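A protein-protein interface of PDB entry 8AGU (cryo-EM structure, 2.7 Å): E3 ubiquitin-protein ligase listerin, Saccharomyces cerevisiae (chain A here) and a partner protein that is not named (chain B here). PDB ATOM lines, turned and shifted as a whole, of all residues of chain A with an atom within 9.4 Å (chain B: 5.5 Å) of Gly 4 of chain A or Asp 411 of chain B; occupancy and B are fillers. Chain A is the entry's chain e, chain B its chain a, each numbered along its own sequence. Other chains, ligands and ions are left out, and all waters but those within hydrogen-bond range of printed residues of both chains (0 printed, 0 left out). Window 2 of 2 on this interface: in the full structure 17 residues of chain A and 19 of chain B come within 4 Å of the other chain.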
ATOM      1  N   SER A   2     -14.333   1.581  23.038  1.00  0.00           N
ATOM      2  CA  SER A   2     -13.109   0.805  22.880  1.00  0.00           C
ATOM      3  C   SER A   2     -11.914   1.728  22.729  1.00  0.00           C
ATOM      4  O   SER A   2     -11.044   1.766  23.595  1.00  0.00           O
ATOM      5  CB  SER A   2     -13.215  -0.124  21.673  1.00  0.00           C
ATOM      6  OG  SER A   2     -12.087  -0.976  21.590  1.00  0.00           O
ATOM      7  N   PHE A   3     -11.859   2.468  21.629  1.00  0.00           N
ATOM      8  CA  PHE A   3     -10.781   3.428  21.438  1.00  0.00           C
ATOM      9  C   PHE A   3     -11.389   4.811  21.311  1.00  0.00           C
ATOM     10  O   PHE A   3     -12.355   4.998  20.577  1.00  0.00           O
ATOM     11  CB  PHE A   3      -9.972   3.098  20.190  1.00  0.00           C
ATOM     12  CG  PHE A   3      -9.317   1.754  20.226  1.00  0.00           C
ATOM     13  CD1 PHE A   3      -8.132   1.567  20.911  1.00  0.00           C
ATOM     14  CD2 PHE A   3      -9.880   0.679  19.563  1.00  0.00           C
ATOM     15  CE1 PHE A   3      -7.519   0.331  20.939  1.00  0.00           C
ATOM     16  CE2 PHE A   3      -9.274  -0.559  19.588  1.00  0.00           C
ATOM     17  CZ  PHE A   3      -8.092  -0.735  20.275  1.00  0.00           C
ATOM     18  N   GLY A   4     -10.844   5.784  22.032  1.00  0.00           N
ATOM     19  CA  GLY A   4     -11.420   7.115  22.011  1.00  0.00           C
ATOM     20  C   GLY A   4     -10.425   8.239  21.844  1.00  0.00           C
ATOM     21  O   GLY A   4      -9.259   8.085  22.192  1.00  0.00           O
ATOM     22  N   GLY A   5     -10.878   9.374  21.320  1.00  0.00           N
ATOM     23  CA  GLY A   5     -10.012  10.531  21.156  1.00  0.00           C
ATOM     24  C   GLY A   5      -9.459  10.778  19.770  1.00  0.00           C
ATOM     25  O   GLY A   5      -9.384   9.861  18.954  1.00  0.00           O
ATOM     26  N   ILE A   6      -9.066  12.018  19.497  1.00  0.00           N
ATOM     27  CA  ILE A   6      -8.549  12.382  18.178  1.00  0.00           C
ATOM     28  C   ILE A   6      -7.178  13.031  18.334  1.00  0.00           C
ATOM     29  O   ILE A   6      -6.977  13.838  19.240  1.00  0.00           O
ATOM     30  CB  ILE A   6      -9.506  13.364  17.469  1.00  0.00           C
ATOM     31  CG1 ILE A   6     -10.839  12.684  17.151  1.00  0.00           C
ATOM     32  CG2 ILE A   6      -8.902  13.898  16.181  1.00  0.00           C
ATOM     33  CD1 ILE A   6     -10.724  11.567  16.136  1.00  0.00           C
ATOM     34  N   ASN A   7      -6.233  12.680  17.466  1.00  0.00           N
ATOM     35  CA  ASN A   7      -4.886  13.236  17.557  1.00  0.00           C
ATOM     36  C   ASN A   7      -4.833  14.589  16.870  1.00  0.00           C
ATOM     37  O   ASN A   7      -4.263  14.710  15.789  1.00  0.00           O
ATOM     38  CB  ASN A   7      -3.872  12.304  16.893  1.00  0.00           C
ATOM     39  CG  ASN A   7      -3.811  10.935  17.544  1.00  0.00           C
ATOM     40  OD1 ASN A   7      -4.637  10.593  18.385  1.00  0.00           O
ATOM     41  ND2 ASN A   7      -2.828  10.138  17.143  1.00  0.00           N
ATOM     42  N   THR A   8      -5.403  15.612  17.498  1.00  0.00           N
ATOM     43  CA  THR A   8      -5.462  16.932  16.877  1.00  0.00           C
ATOM     44  C   THR A   8      -4.094  17.541  16.620  1.00  0.00           C
ATOM     45  O   THR A   8      -3.857  18.095  15.553  1.00  0.00           O
ATOM     46  CB  THR A   8      -6.252  17.911  17.757  1.00  0.00           C
ATOM     47  OG1 THR A   8      -5.620  18.013  19.038  1.00  0.00           O
ATOM     48  CG2 THR A   8      -7.678  17.427  17.943  1.00  0.00           C
ATOM     49  N   PRO A  34      -0.696   4.646  17.224  1.00  0.00           N
ATOM     50  CA  PRO A  34      -1.793   4.511  16.260  1.00  0.00           C
ATOM     51  C   PRO A  34      -3.019   5.313  16.669  1.00  0.00           C
ATOM     52  O   PRO A  34      -3.378   5.324  17.845  1.00  0.00           O
ATOM     53  CB  PRO A  34      -2.108   3.017  16.297  1.00  0.00           C
ATOM     54  CG  PRO A  34      -0.861   2.370  16.799  1.00  0.00           C
ATOM     55  CD  PRO A  34      -0.265   3.348  17.765  1.00  0.00           C
ATOM     56  N   ASP A  35      -3.660   5.971  15.708  1.00  0.00           N
ATOM     57  CA  ASP A  35      -4.827   6.796  16.008  1.00  0.00           C
ATOM     58  C   ASP A  35      -5.960   5.931  16.522  1.00  0.00           C
ATOM     59  O   ASP A  35      -6.204   4.847  16.000  1.00  0.00           O
ATOM     60  CB  ASP A  35      -5.275   7.544  14.749  1.00  0.00           C
ATOM     61  CG  ASP A  35      -6.157   8.742  15.057  1.00  0.00           C
ATOM     62  OD1 ASP A  35      -7.360   8.553  15.329  1.00  0.00           O
ATOM     63  OD2 ASP A  35      -5.646   9.879  15.023  1.00  0.00           O
ATOM     64  N   PRO A  36      -6.677   6.421  17.535  1.00  0.00           N
ATOM     65  CA  PRO A  36      -7.761   5.629  18.112  1.00  0.00           C
ATOM     66  C   PRO A  36      -8.851   5.317  17.097  1.00  0.00           C
ATOM     67  O   PRO A  36      -9.379   4.209  17.093  1.00  0.00           O
ATOM     68  CB  PRO A  36      -8.307   6.546  19.198  1.00  0.00           C
ATOM     69  CG  PRO A  36      -7.118   7.326  19.637  1.00  0.00           C
ATOM     70  CD  PRO A  36      -6.322   7.568  18.389  1.00  0.00           C
ATOM     71  N   SER A  37      -9.192   6.279  16.249  1.00  0.00           N
ATOM     72  CA  SER A  37     -10.255   6.061  15.280  1.00  0.00           C
ATOM     73  C   SER A  37      -9.878   4.946  14.323  1.00  0.00           C
ATOM     74  O   SER A  37     -10.708   4.103  13.985  1.00  0.00           O
ATOM     75  CB  SER A  37     -10.538   7.342  14.498  1.00  0.00           C
ATOM     76  OG  SER A  37      -9.436   7.699  13.682  1.00  0.00           O
ATOM     77  N   LEU A  38      -8.625   4.933  13.891  1.00  0.00           N
ATOM     78  CA  LEU A  38      -8.166   3.895  12.983  1.00  0.00           C
ATOM     79  C   LEU A  38      -8.257   2.554  13.680  1.00  0.00           C
ATOM     80  O   LEU A  38      -8.624   1.550  13.070  1.00  0.00           O
ATOM     81  CB  LEU A  38      -6.731   4.174  12.541  1.00  0.00           C
ATOM     82  CG  LEU A  38      -6.262   3.506  11.245  1.00  0.00           C
ATOM     83  CD1 LEU A  38      -7.166   3.903  10.087  1.00  0.00           C
ATOM     84  CD2 LEU A  38      -4.816   3.869  10.943  1.00  0.00           C
ATOM     85  N   LEU A  39      -7.917   2.531  14.962  1.00  0.00           N
ATOM     86  CA  LEU A  39      -7.979   1.294  15.728  1.00  0.00           C
ATOM     87  C   LEU A  39      -9.403   0.770  15.810  1.00  0.00           C
ATOM     88  O   LEU A  39      -9.624  -0.435  15.724  1.00  0.00           O
ATOM     89  CB  LEU A  39      -7.382   1.506  17.114  1.00  0.00           C
ATOM     90  CG  LEU A  39      -5.864   1.672  17.142  1.00  0.00           C
ATOM     91  CD1 LEU A  39      -5.382   2.246  18.464  1.00  0.00           C
ATOM     92  CD2 LEU A  39      -5.179   0.349  16.835  1.00  0.00           C
ATOM     93  N   ASN A  40     -10.374   1.660  15.966  1.00  0.00           N
ATOM     94  CA  ASN A  40     -11.774   1.246  15.979  1.00  0.00           C
ATOM     95  C   ASN A  40     -12.115   0.625  14.643  1.00  0.00           C
ATOM     96  O   ASN A  40     -12.898  -0.317  14.574  1.00  0.00           O
ATOM     97  CB  ASN A  40     -12.683   2.440  16.226  1.00  0.00           C
ATOM     98  CG  ASN A  40     -12.630   2.924  17.656  1.00  0.00           C
ATOM     99  OD1 ASN A  40     -12.775   2.140  18.593  1.00  0.00           O
ATOM    100  ND2 ASN A  40     -12.436   4.224  17.831  1.00  0.00           N
ATOM    101  N   LYS A  52      -4.068  -3.426  21.834  1.00  0.00           N
ATOM    102  CA  LYS A  52      -4.060  -2.809  23.151  1.00  0.00           C
ATOM    103  C   LYS A  52      -2.946  -3.397  23.991  1.00  0.00           C
ATOM    104  O   LYS A  52      -2.266  -2.680  24.717  1.00  0.00           O
ATOM    105  CB  LYS A  52      -5.382  -3.042  23.870  1.00  0.00           C
ATOM    106  CG  LYS A  52      -6.563  -2.259  23.333  1.00  0.00           C
ATOM    107  CD  LYS A  52      -7.822  -2.600  24.113  1.00  0.00           C
ATOM    108  CE  LYS A  52      -9.016  -1.784  23.649  1.00  0.00           C
ATOM    109  NZ  LYS A  52     -10.254  -2.118  24.404  1.00  0.00           N
ATOM    110  N   VAL B 406      -6.166  19.688  23.595  1.00  0.00           N
ATOM    111  CA  VAL B 406      -5.696  19.052  24.814  1.00  0.00           C
ATOM    112  C   VAL B 406      -6.671  17.973  25.223  1.00  0.00           C
ATOM    113  O   VAL B 406      -6.272  16.886  25.635  1.00  0.00           O
ATOM    114  CB  VAL B 406      -5.509  20.065  25.955  1.00  0.00           C
ATOM    115  CG1 VAL B 406      -4.945  19.380  27.190  1.00  0.00           C
ATOM    116  CG2 VAL B 406      -4.576  21.180  25.516  1.00  0.00           C
ATOM    117  N   GLN B 407      -7.957  18.251  25.068  1.00  0.00           N
ATOM    118  CA  GLN B 407      -8.963  17.301  25.503  1.00  0.00           C
ATOM    119  C   GLN B 407      -8.810  16.005  24.746  1.00  0.00           C
ATOM    120  O   GLN B 407      -8.969  14.935  25.312  1.00  0.00           O
ATOM    121  CB  GLN B 407     -10.366  17.866  25.315  1.00  0.00           C
ATOM    122  CG  GLN B 407     -11.435  17.112  26.086  1.00  0.00           C
ATOM    123  CD  GLN B 407     -11.172  17.102  27.580  1.00  0.00           C
ATOM    124  OE1 GLN B 407     -11.203  16.051  28.218  1.00  0.00           O
ATOM    125  NE2 GLN B 407     -10.901  18.275  28.144  1.00  0.00           N
ATOM    126  N   GLY B 408      -8.486  16.094  23.463  1.00  0.00           N
ATOM    127  CA  GLY B 408      -8.360  14.898  22.662  1.00  0.00           C
ATOM    128  C   GLY B 408      -7.269  14.005  23.205  1.00  0.00           C
ATOM    129  O   GLY B 408      -7.433  12.788  23.276  1.00  0.00           O
ATOM    130  N   LEU B 409      -6.156  14.599  23.608  1.00  0.00           N
ATOM    131  CA  LEU B 409      -5.084  13.810  24.199  1.00  0.00           C
ATOM    132  C   LEU B 409      -5.528  13.156  25.497  1.00  0.00           C
ATOM    133  O   LEU B 409      -5.218  11.994  25.747  1.00  0.00           O
ATOM    134  CB  LEU B 409      -3.853  14.680  24.450  1.00  0.00           C
ATOM    135  CG  LEU B 409      -2.839  14.862  23.318  1.00  0.00           C
ATOM    136  CD1 LEU B 409      -2.314  13.516  22.854  1.00  0.00           C
ATOM    137  CD2 LEU B 409      -3.408  15.639  22.145  1.00  0.00           C
ATOM    138  N   ILE B 410      -6.256  13.896  26.325  1.00  0.00           N
ATOM    139  CA  ILE B 410      -6.735  13.358  27.593  1.00  0.00           C
ATOM    140  C   ILE B 410      -7.689  12.205  27.347  1.00  0.00           C
ATOM    141  O   ILE B 410      -7.639  11.191  28.037  1.00  0.00           O
ATOM    142  CB  ILE B 410      -7.435  14.446  28.423  1.00  0.00           C
ATOM    143  CG1 ILE B 410      -6.481  15.607  28.682  1.00  0.00           C
ATOM    144  CG2 ILE B 410      -7.936  13.893  29.748  1.00  0.00           C
ATOM    145  CD1 ILE B 410      -7.101  16.724  29.486  1.00  0.00           C
ATOM    146  N   ASP B 411      -8.544  12.344  26.344  1.00  0.00           N
ATOM    147  CA  ASP B 411      -9.504  11.297  26.022  1.00  0.00           C
ATOM    148  C   ASP B 411      -8.767  10.043  25.623  1.00  0.00           C
ATOM    149  O   ASP B 411      -9.200   8.937  25.931  1.00  0.00           O
ATOM    150  CB  ASP B 411     -10.435  11.747  24.905  1.00  0.00           C
ATOM    151  CG  ASP B 411     -11.318  12.904  25.320  1.00  0.00           C
ATOM    152  OD1 ASP B 411     -11.392  13.187  26.534  1.00  0.00           O
ATOM    153  OD2 ASP B 411     -11.934  13.534  24.436  1.00  0.00           O
ATOM    154  N   GLN B 412      -7.650  10.209  24.933  1.00  0.00           N
ATOM    155  CA  GLN B 412      -6.852   9.069  24.521  1.00  0.00           C
ATOM    156  C   GLN B 412      -6.348   8.314  25.739  1.00  0.00           C
ATOM    157  O   GLN B 412      -6.115   7.111  25.672  1.00  0.00           O
ATOM    158  CB  GLN B 412      -5.691   9.529  23.650  1.00  0.00           C
ATOM    159  CG  GLN B 412      -6.130  10.400  22.487  1.00  0.00           C
ATOM    160  CD  GLN B 412      -4.966  10.885  21.652  1.00  0.00           C
ATOM    161  OE1 GLN B 412      -3.900  10.271  21.633  1.00  0.00           O
ATOM    162  NE2 GLN B 412      -5.167  11.992  20.950  1.00  0.00           N
ATOM    163  N   GLN B 413      -6.182   9.012  26.856  1.00  0.00           N
ATOM    164  CA  GLN B 413      -5.690   8.373  28.069  1.00  0.00           C
ATOM    165  C   GLN B 413      -4.186   8.290  28.088  1.00  0.00           C
ATOM    166  O   GLN B 413      -3.612   7.486  28.816  1.00  0.00           O
ATOM    167  CB  GLN B 413      -6.293   6.983  28.231  1.00  0.00           C
ATOM    168  CG  GLN B 413      -7.716   6.986  28.764  1.00  0.00           C
ATOM    169  CD  GLN B 413      -8.233   5.591  29.041  1.00  0.00           C
ATOM    170  OE1 GLN B 413      -9.390   5.407  29.416  1.00  0.00           O
ATOM    171  NE2 GLN B 413      -7.373   4.595  28.858  1.00  0.00           N
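NE2 of Gln 412 of chain B is in hydrogen-bond range of O of Ile 6 of chain A, 3.1 Å away. NE2 of Gln 412 of chain B is in hydrogen-bond range of OD1 of Asn 7 of chain A, at 3.0 Å.
The side-chain amide oxygen of Gln 407 of chain B lies close to the side-chain carboxylate of Asp 411 of chain B (3.3 Å). The backbone carbonyl oxygen of Gly 408 of chain B sits close to the side-chain amide nitrogen of Gln 412 of chain B, 3.3 Å away.
Among the printed residues, pairs that only touch across the chains: Gly 4 of chain A with Gln 412 of chain B, Gly 4 of chain A with Asp 411 of chain B, Ile 6 of chain A with Gly 408 of chain B and Gly 5 of chain A with Asp 411 of chain B.
Printed residues of chain B within 4 Å of Gly 5 of chain A: Asp 411 (3.96 Å). Of the printed residues of chain B, Asn 7 of chain A touches Gln 412 (3.0 Å). Gly 408 of chain B touches just one residue of chain A: Ile 6 (3.8 Å). Asp 411 of chain B touches two residues of chain A. Of the printed residues of chain A, Gln 412 of chain B touches Gly 4, Ile 6 and Asn 7. The nearest residue of chain B that does not touch Gly 4 of chain A is Gly 408 of chain B (5.2 Å). The nearest residue of chain A that does not touch Asp 411 of chain B is Ile 6 of chain A (5.6 Å). The nearest printed residue of chain B that does not touch Gly 5 of chain A is Gly 408 of chain B (4.03 Å).
Among the printed residues, no Asp or Glu carboxylate lies within 4 Å of a Lys or Arg side-chain nitrogen of the other chain.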
